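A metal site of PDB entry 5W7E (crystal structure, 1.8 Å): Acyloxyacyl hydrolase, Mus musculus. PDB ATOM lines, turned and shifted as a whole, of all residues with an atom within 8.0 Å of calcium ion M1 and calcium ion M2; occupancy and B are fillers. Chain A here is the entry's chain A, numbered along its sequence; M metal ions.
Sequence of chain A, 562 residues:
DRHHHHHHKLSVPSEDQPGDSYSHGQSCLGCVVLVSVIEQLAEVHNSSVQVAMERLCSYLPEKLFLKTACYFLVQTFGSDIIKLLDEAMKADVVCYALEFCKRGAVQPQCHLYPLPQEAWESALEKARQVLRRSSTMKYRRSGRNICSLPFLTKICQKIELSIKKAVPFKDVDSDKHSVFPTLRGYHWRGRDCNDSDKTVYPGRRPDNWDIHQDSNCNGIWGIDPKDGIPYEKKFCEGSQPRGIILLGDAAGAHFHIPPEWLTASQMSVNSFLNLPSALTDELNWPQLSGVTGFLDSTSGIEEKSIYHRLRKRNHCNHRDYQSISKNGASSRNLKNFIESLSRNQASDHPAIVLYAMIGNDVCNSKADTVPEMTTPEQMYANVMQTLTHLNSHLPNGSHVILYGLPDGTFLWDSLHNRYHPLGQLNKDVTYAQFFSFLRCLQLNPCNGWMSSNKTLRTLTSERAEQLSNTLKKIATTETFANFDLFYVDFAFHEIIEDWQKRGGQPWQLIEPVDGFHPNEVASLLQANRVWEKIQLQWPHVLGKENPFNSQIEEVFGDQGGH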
ATOM      1  N   PRO A 168     -10.765  16.143 -24.314  1.00  0.00           N
ATOM      2  CA  PRO A 168     -10.813  15.696 -22.929  1.00  0.00           C
ATOM      3  C   PRO A 168     -11.483  16.705 -22.008  1.00  0.00           C
ATOM      4  O   PRO A 168     -11.222  17.910 -22.076  1.00  0.00           O
ATOM      5  CB  PRO A 168      -9.333  15.511 -22.566  1.00  0.00           C
ATOM      6  CG  PRO A 168      -8.598  16.304 -23.581  1.00  0.00           C
ATOM      7  CD  PRO A 168      -9.385  16.152 -24.821  1.00  0.00           C
ATOM      8  N   LYS A 170     -11.041  16.735 -18.715  1.00  0.00           N
ATOM      9  CA  LYS A 170      -9.977  17.158 -17.797  1.00  0.00           C
ATOM     10  C   LYS A 170      -8.744  17.502 -18.635  1.00  0.00           C
ATOM     11  O   LYS A 170      -8.081  16.613 -19.174  1.00  0.00           O
ATOM     12  CB  LYS A 170      -9.666  16.059 -16.787  1.00  0.00           C
ATOM     13  CG  LYS A 170     -10.873  15.481 -16.079  1.00  0.00           C
ATOM     14  CD  LYS A 170     -11.308  16.268 -14.858  1.00  0.00           C
ATOM     15  CE  LYS A 170     -11.539  15.345 -13.643  1.00  0.00           C
ATOM     16  NZ  LYS A 170     -12.515  14.218 -13.870  1.00  0.00           N
ATOM     17  N   ASP A 171      -8.434  18.801 -18.725  1.00  0.00           N
ATOM     18  CA  ASP A 171      -7.370  19.312 -19.575  1.00  0.00           C
ATOM     19  C   ASP A 171      -7.075  20.753 -19.185  1.00  0.00           C
ATOM     20  O   ASP A 171      -7.520  21.697 -19.847  1.00  0.00           O
ATOM     21  CB  ASP A 171      -7.784  19.162 -21.041  1.00  0.00           C
ATOM     22  CG  ASP A 171      -6.691  19.557 -22.016  1.00  0.00           C
ATOM     23  OD1 ASP A 171      -7.077  19.830 -23.176  1.00  0.00           O
ATOM     24  OD2 ASP A 171      -5.477  19.608 -21.636  1.00  0.00           O
ATOM     25  N   VAL A 172      -6.299  20.926 -18.101  1.00  0.00           N
ATOM     26  CA  VAL A 172      -6.075  22.247 -17.510  1.00  0.00           C
ATOM     27  C   VAL A 172      -5.424  23.178 -18.523  1.00  0.00           C
ATOM     28  O   VAL A 172      -5.813  24.349 -18.630  1.00  0.00           O
ATOM     29  CB  VAL A 172      -5.231  22.133 -16.244  1.00  0.00           C
ATOM     30  CG1 VAL A 172      -4.769  23.516 -15.755  1.00  0.00           C
ATOM     31  CG2 VAL A 172      -6.014  21.449 -15.175  1.00  0.00           C
ATOM     32  N   ASP A 173      -4.407  22.697 -19.243  1.00  0.00           N
ATOM     33  CA  ASP A 173      -3.681  23.565 -20.165  1.00  0.00           C
ATOM     34  C   ASP A 173      -4.240  23.533 -21.581  1.00  0.00           C
ATOM     35  O   ASP A 173      -3.637  24.140 -22.478  1.00  0.00           O
ATOM     36  CB  ASP A 173      -2.184  23.210 -20.186  1.00  0.00           C
ATOM     37  CG  ASP A 173      -1.936  21.823 -20.718  1.00  0.00           C
ATOM     38  OD1 ASP A 173      -2.892  21.212 -21.219  1.00  0.00           O
ATOM     39  OD2 ASP A 173      -0.784  21.359 -20.618  1.00  0.00           O
ATOM     40  N   SER A 174      -5.347  22.819 -21.801  1.00  0.00           N
ATOM     41  CA  SER A 174      -6.126  22.874 -23.046  1.00  0.00           C
ATOM     42  C   SER A 174      -5.371  22.357 -24.264  1.00  0.00           C
ATOM     43  O   SER A 174      -5.718  22.721 -25.397  1.00  0.00           O
ATOM     44  CB  SER A 174      -6.635  24.292 -23.317  1.00  0.00           C
ATOM     45  OG  SER A 174      -7.603  24.698 -22.353  1.00  0.00           O
ATOM     46  N   ASP A 175      -4.348  21.513 -24.102  1.00  0.00           N
ATOM     47  CA  ASP A 175      -3.628  20.988 -25.268  1.00  0.00           C
ATOM     48  C   ASP A 175      -4.238  19.690 -25.806  1.00  0.00           C
ATOM     49  O   ASP A 175      -3.629  19.050 -26.671  1.00  0.00           O
ATOM     50  CB  ASP A 175      -2.124  20.831 -24.957  1.00  0.00           C
ATOM     51  CG  ASP A 175      -1.820  19.887 -23.811  1.00  0.00           C
ATOM     52  OD1 ASP A 175      -2.716  19.101 -23.411  1.00  0.00           O
ATOM     53  OD2 ASP A 175      -0.664  19.939 -23.304  1.00  0.00           O
ATOM     54  N   LYS A 176      -5.428  19.311 -25.329  1.00  0.00           N
ATOM     55  CA  LYS A 176      -6.217  18.142 -25.752  1.00  0.00           C
ATOM     56  C   LYS A 176      -5.628  16.814 -25.286  1.00  0.00           C
ATOM     57  O   LYS A 176      -6.104  15.738 -25.702  1.00  0.00           O
ATOM     58  CB  LYS A 176      -6.414  18.127 -27.274  1.00  0.00           C
ATOM     59  CG  LYS A 176      -7.300  19.285 -27.757  1.00  0.00           C
ATOM     60  CD  LYS A 176      -7.518  19.289 -29.258  1.00  0.00           C
ATOM     61  CE  LYS A 176      -8.232  20.543 -29.725  1.00  0.00           C
ATOM     62  NZ  LYS A 176      -7.457  21.784 -29.402  1.00  0.00           N
ATOM     63  N   HIS A 177      -4.626  16.834 -24.403  1.00  0.00           N
ATOM     64  CA  HIS A 177      -4.089  15.643 -23.778  1.00  0.00           C
ATOM     65  C   HIS A 177      -4.357  15.717 -22.283  1.00  0.00           C
ATOM     66  O   HIS A 177      -4.220  16.779 -21.675  1.00  0.00           O
ATOM     67  CB  HIS A 177      -2.579  15.493 -24.077  1.00  0.00           C
ATOM     68  CG  HIS A 177      -2.297  15.216 -25.511  1.00  0.00           C
ATOM     69  ND1 HIS A 177      -2.147  13.940 -26.009  1.00  0.00           N
ATOM     70  CD2 HIS A 177      -2.170  16.054 -26.571  1.00  0.00           C
ATOM     71  CE1 HIS A 177      -1.922  14.001 -27.305  1.00  0.00           C
ATOM     72  NE2 HIS A 177      -1.929  15.269 -27.670  1.00  0.00           N
ATOM     73  N   SER A 178      -4.732  14.592 -21.702  1.00  0.00           N
ATOM     74  CA  SER A 178      -5.250  14.557 -20.345  1.00  0.00           C
ATOM     75  C   SER A 178      -4.375  13.713 -19.424  1.00  0.00           C
ATOM     76  O   SER A 178      -3.582  12.877 -19.859  1.00  0.00           O
ATOM     77  CB  SER A 178      -6.673  13.998 -20.366  1.00  0.00           C
ATOM     78  OG  SER A 178      -7.321  14.074 -19.102  1.00  0.00           O
ATOM     79  N   VAL A 179      -4.551  13.947 -18.118  1.00  0.00           N
ATOM     80  CA  VAL A 179      -4.004  13.062 -17.086  1.00  0.00           C
ATOM     81  C   VAL A 179      -5.045  12.074 -16.577  1.00  0.00           C
ATOM     82  O   VAL A 179      -4.730  11.217 -15.743  1.00  0.00           O
ATOM     83  CB  VAL A 179      -3.422  13.872 -15.909  1.00  0.00           C
ATOM     84  CG1 VAL A 179      -2.479  14.931 -16.406  1.00  0.00           C
ATOM     85  CG2 VAL A 179      -4.537  14.511 -15.084  1.00  0.00           C
ATOM     86  N   GLY A 190      -2.250  10.038 -26.093  1.00  0.00           N
ATOM     87  CA  GLY A 190      -1.153  10.006 -25.168  1.00  0.00           C
ATOM     88  C   GLY A 190      -1.370  10.872 -23.938  1.00  0.00           C
ATOM     89  O   GLY A 190      -1.837  12.011 -24.050  1.00  0.00           O
ATOM     90  N   ARG A 191      -1.038  10.317 -22.784  1.00  0.00           N
ATOM     91  CA  ARG A 191      -1.193  11.002 -21.508  1.00  0.00           C
ATOM     92  C   ARG A 191      -0.283  12.227 -21.437  1.00  0.00           C
ATOM     93  O   ARG A 191       0.897  12.160 -21.794  1.00  0.00           O
ATOM     94  CB  ARG A 191      -0.880  10.037 -20.362  1.00  0.00           C
ATOM     95  CG  ARG A 191      -1.292  10.586 -18.981  1.00  0.00           C
ATOM     96  CD  ARG A 191      -0.555   9.926 -17.844  1.00  0.00           C
ATOM     97  NE  ARG A 191      -0.828   8.496 -17.739  1.00  0.00           N
ATOM     98  CZ  ARG A 191      -1.456   7.888 -16.728  1.00  0.00           C
ATOM     99  NH1 ARG A 191      -1.902   8.572 -15.682  1.00  0.00           N
ATOM    100  NH2 ARG A 191      -1.629   6.584 -16.744  1.00  0.00           N
ATOM    101  N   ASP A 192      -0.839  13.347 -20.988  1.00  0.00           N
ATOM    102  CA  ASP A 192      -0.090  14.601 -20.808  1.00  0.00           C
ATOM    103  C   ASP A 192       0.882  14.472 -19.648  1.00  0.00           C
ATOM    104  O   ASP A 192       0.459  14.288 -18.503  1.00  0.00           O
ATOM    105  CB  ASP A 192      -1.064  15.749 -20.552  1.00  0.00           C
ATOM    106  CG  ASP A 192      -0.464  17.102 -20.803  1.00  0.00           C
ATOM    107  OD1 ASP A 192       0.783  17.204 -20.858  1.00  0.00           O
ATOM    108  OD2 ASP A 192      -1.264  18.069 -20.927  1.00  0.00           O
ATOM    109  N   CYS A 193       2.179  14.606 -19.927  1.00  0.00           N
ATOM    110  CA  CYS A 193       3.190  14.565 -18.879  1.00  0.00           C
ATOM    111  C   CYS A 193       3.224  15.856 -18.055  1.00  0.00           C
ATOM    112  O   CYS A 193       3.681  15.836 -16.900  1.00  0.00           O
ATOM    113  CB  CYS A 193       4.583  14.247 -19.471  1.00  0.00           C
ATOM    114  SG  CYS A 193       5.171  15.219 -20.934  1.00  0.00           S
ATOM    115  N   ASN A 194       2.724  16.962 -18.594  1.00  0.00           N
ATOM    116  CA  ASN A 194       2.611  18.216 -17.836  1.00  0.00           C
ATOM    117  C   ASN A 194       1.334  18.920 -18.264  1.00  0.00           C
ATOM    118  O   ASN A 194       1.306  19.581 -19.303  1.00  0.00           O
ATOM    119  CB  ASN A 194       3.840  19.093 -18.051  1.00  0.00           C
ATOM    120  CG  ASN A 194       3.917  20.215 -17.023  1.00  0.00           C
ATOM    121  OD1 ASN A 194       2.893  20.600 -16.471  1.00  0.00           O
ATOM    122  ND2 ASN A 194       5.126  20.708 -16.768  1.00  0.00           N
ATOM    123  N   ASP A 195       0.272  18.789 -17.471  1.00  0.00           N
ATOM    124  CA  ASP A 195      -1.011  19.401 -17.770  1.00  0.00           C
ATOM    125  C   ASP A 195      -1.059  20.873 -17.369  1.00  0.00           C
ATOM    126  O   ASP A 195      -2.128  21.494 -17.451  1.00  0.00           O
ATOM    127  CB  ASP A 195      -2.126  18.624 -17.086  1.00  0.00           C
ATOM    128  CG  ASP A 195      -3.491  18.868 -17.715  1.00  0.00           C
ATOM    129  OD1 ASP A 195      -3.581  19.051 -18.952  1.00  0.00           O
ATOM    130  OD2 ASP A 195      -4.496  18.854 -16.969  1.00  0.00           O
ATOM    131  N   SER A 196       0.072  21.425 -16.915  1.00  0.00           N
ATOM    132  CA  SER A 196       0.241  22.841 -16.641  1.00  0.00           C
ATOM    133  C   SER A 196       1.166  23.496 -17.653  1.00  0.00           C
ATOM    134  O   SER A 196       1.851  24.462 -17.339  1.00  0.00           O
ATOM    135  CB  SER A 196       0.791  23.067 -15.223  1.00  0.00           C
ATOM    136  OG  SER A 196       0.018  22.378 -14.255  1.00  0.00           O
ATOM    137  N   ASP A 197       1.223  22.951 -18.864  1.00  0.00           N
ATOM    138  CA  ASP A 197       2.094  23.531 -19.896  1.00  0.00           C
ATOM    139  C   ASP A 197       1.568  23.071 -21.244  1.00  0.00           C
ATOM    140  O   ASP A 197       1.736  21.901 -21.603  1.00  0.00           O
ATOM    141  CB  ASP A 197       3.543  23.120 -19.687  1.00  0.00           C
ATOM    142  CG  ASP A 197       4.507  23.892 -20.580  1.00  0.00           C
ATOM    143  OD1 ASP A 197       4.069  24.349 -21.666  1.00  0.00           O
ATOM    144  OD2 ASP A 197       5.690  24.046 -20.193  1.00  0.00           O
ATOM    145  N   LYS A 198       0.950  23.994 -21.975  1.00  0.00           N
ATOM    146  CA  LYS A 198       0.373  23.707 -23.282  1.00  0.00           C
ATOM    147  C   LYS A 198       1.426  23.444 -24.359  1.00  0.00           C
ATOM    148  O   LYS A 198       1.062  23.067 -25.474  1.00  0.00           O
ATOM    149  CB  LYS A 198      -0.537  24.857 -23.703  1.00  0.00           C
ATOM    150  CG  LYS A 198       0.162  26.195 -23.903  1.00  0.00           C
ATOM    151  CD  LYS A 198      -0.779  27.242 -24.489  1.00  0.00           C
ATOM    152  CE  LYS A 198      -0.025  28.425 -25.119  1.00  0.00           C
ATOM    153  NZ  LYS A 198       0.525  29.379 -24.101  1.00  0.00           N
ATOM    154  N   THR A 199       2.700  23.610 -24.070  1.00  0.00           N
ATOM    155  CA  THR A 199       3.736  23.266 -25.037  1.00  0.00           C
ATOM    156  C   THR A 199       4.387  21.934 -24.741  1.00  0.00           C
ATOM    157  O   THR A 199       5.339  21.550 -25.431  1.00  0.00           O
ATOM    158  CB  THR A 199       4.809  24.370 -25.094  1.00  0.00           C
ATOM    159  OG1 THR A 199       5.468  24.470 -23.830  1.00  0.00           O
ATOM    160  CG2 THR A 199       4.172  25.701 -25.453  1.00  0.00           C
ATOM    161  N   VAL A 200       3.894  21.217 -23.740  1.00  0.00           N
ATOM    162  CA  VAL A 200       4.357  19.883 -23.379  1.00  0.00           C
ATOM    163  C   VAL A 200       3.205  18.922 -23.641  1.00  0.00           C
ATOM    164  O   VAL A 200       2.153  19.023 -22.992  1.00  0.00           O
ATOM    165  CB  VAL A 200       4.790  19.809 -21.906  1.00  0.00           C
ATOM    166  CG1 VAL A 200       5.114  18.383 -21.524  1.00  0.00           C
ATOM    167  CG2 VAL A 200       6.001  20.719 -21.655  1.00  0.00           C
ATOM    168  N   TYR A 201       3.391  18.011 -24.586  1.00  0.00           N
ATOM    169  CA  TYR A 201       2.379  17.021 -24.948  1.00  0.00           C
ATOM    170  C   TYR A 201       2.992  16.058 -25.967  1.00  0.00           C
ATOM    171  O   TYR A 201       3.931  16.426 -26.685  1.00  0.00           O
ATOM    172  CB  TYR A 201       1.126  17.689 -25.541  1.00  0.00           C
ATOM    173  CG  TYR A 201       1.429  18.575 -26.730  1.00  0.00           C
ATOM    174  CD1 TYR A 201       1.647  18.039 -27.999  1.00  0.00           C
ATOM    175  CD2 TYR A 201       1.525  19.952 -26.585  1.00  0.00           C
ATOM    176  CE1 TYR A 201       1.940  18.847 -29.084  1.00  0.00           C
ATOM    177  CE2 TYR A 201       1.814  20.763 -27.658  1.00  0.00           C
ATOM    178  CZ  TYR A 201       2.025  20.203 -28.901  1.00  0.00           C
ATOM    179  OH  TYR A 201       2.308  21.021 -29.977  1.00  0.00           O
ATOM    180  N   PRO A 202       2.439  14.841 -26.090  1.00  0.00           N
ATOM    181  CA  PRO A 202       2.988  13.870 -27.057  1.00  0.00           C
ATOM    182  C   PRO A 202       2.937  14.361 -28.491  1.00  0.00           C
ATOM    183  O   PRO A 202       1.941  14.927 -28.945  1.00  0.00           O
ATOM    184  CB  PRO A 202       2.094  12.642 -26.847  1.00  0.00           C
ATOM    185  CG  PRO A 202       1.533  12.795 -25.496  1.00  0.00           C
ATOM    186  CD  PRO A 202       1.374  14.260 -25.263  1.00  0.00           C
ATOM    187  N   GLN A 213      13.443  19.369 -19.696  1.00  0.00           N
ATOM    188  CA  GLN A 213      12.121  18.796 -19.510  1.00  0.00           C
ATOM    189  C   GLN A 213      11.812  17.862 -20.665  1.00  0.00           C
ATOM    190  O   GLN A 213      12.272  18.058 -21.796  1.00  0.00           O
ATOM    191  CB  GLN A 213      11.041  19.890 -19.411  1.00  0.00           C
ATOM    192  CG  GLN A 213       9.670  19.297 -19.069  1.00  0.00           C
ATOM    193  CD  GLN A 213       8.586  20.333 -18.773  1.00  0.00           C
ATOM    194  OE1 GLN A 213       7.532  19.981 -18.230  1.00  0.00           O
ATOM    195  NE2 GLN A 213       8.835  21.598 -19.132  1.00  0.00           N
ATOM    196  N   SER A 215       9.561  17.460 -23.014  1.00  0.00           N
ATOM    197  CA  SER A 215       8.505  18.280 -23.611  1.00  0.00           C
ATOM    198  C   SER A 215       7.553  17.493 -24.514  1.00  0.00           C
ATOM    199  O   SER A 215       6.453  17.983 -24.792  1.00  0.00           O
ATOM    200  CB  SER A 215       9.113  19.449 -24.388  1.00  0.00           C
ATOM    201  OG  SER A 215       9.772  18.989 -25.568  1.00  0.00           O
ATOM    202  N   CYS A 217       6.754  14.077 -23.925  1.00  0.00           N
ATOM    203  CA  CYS A 217       6.148  12.999 -23.145  1.00  0.00           C
ATOM    204  C   CYS A 217       6.562  11.607 -23.581  1.00  0.00           C
ATOM    205  O   CYS A 217       5.896  10.625 -23.231  1.00  0.00           O
ATOM    206  CB  CYS A 217       4.617  13.097 -23.175  1.00  0.00           C
ATOM    207  SG  CYS A 217       4.016  14.687 -22.612  1.00  0.00           S
HETATM  208 CA    CA M   1       0.595  19.688 -21.472  1.00  0.00          CA
HETATM  209 CA    CA M   2      -3.380  18.916 -21.218  1.00  0.00          CA
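The side-chain amide oxygen (OD1) of Asn 194 is in hydrogen-bond range of the backbone NH (N) of Ser 196 (3.0 Å).
The side-chain carboxylate (OD2) of Asp 173 lies close to the backbone NH (N) of Lys 198 (3.4 Å).
ND2 of Asn 194 lies within hydrogen-bond range of OE1 of Gln 213 (2.9 Å).
The side-chain carboxylate of Asp 171 lies close to the backbone NH of Ser 174.
N of Asp 192 lies within hydrogen-bond range of O of Ser 178.
The side-chain carboxylate (OD1) of Asp 171 lies within hydrogen-bond range of the backbone NH (N) of Lys 176 (2.8 Å).
A ring nitrogen (ND1) of His 177 sits at hydrogen-bond distance from the backbone carbonyl oxygen of Gly 190.
OD2 of Asp 195 lies within hydrogen-bond range of N of Val 172 (3.0 Å).
Of the 27 residues printed, 6 come within 4 Å of calcium ion M1.
Of the 27 residues printed, 6 come within 4 Å of calcium ion M2.
The nearest printed residue that does not touch calcium ion M2 is Ser 174 (4.4 Å).
Calcium ion M1 is bound by the side-chain carboxylate (OD2) of Asp 175 (2.2 Å), the backbone carbonyl oxygen (O) of Val 200 (2.3 Å), the backbone carbonyl oxygen (O) of Asn 194 (2.3 Å), the side-chain carboxylate (OD2) of Asp 173 (2.3 Å), the backbone carbonyl oxygen (O) of Asp 197 (2.5 Å), the side-chain carboxylate (OD2) of Asp 192 (2.5 Å) and the side-chain carboxylate (OD1) of Asp 192 (2.6 Å).
OD2 of Asp 171 is bound to calcium ion M2 (2.2 Å).
The side-chain carboxylate (OD1) of Asp 195 is bound to calcium ion M2.
The side-chain carboxylate (OD2) of Asp 192 is bound to calcium ion M2 (2.3 Å).
Calcium ion M2 is bound by the side-chain carboxylate (OD1) of Asp 175 (2.3 Å).
O of His 177 is bound to calcium ion M2 (2.3 Å).
Calcium ion M2 is bound by OD1 of Asp 173 (2.3 Å).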
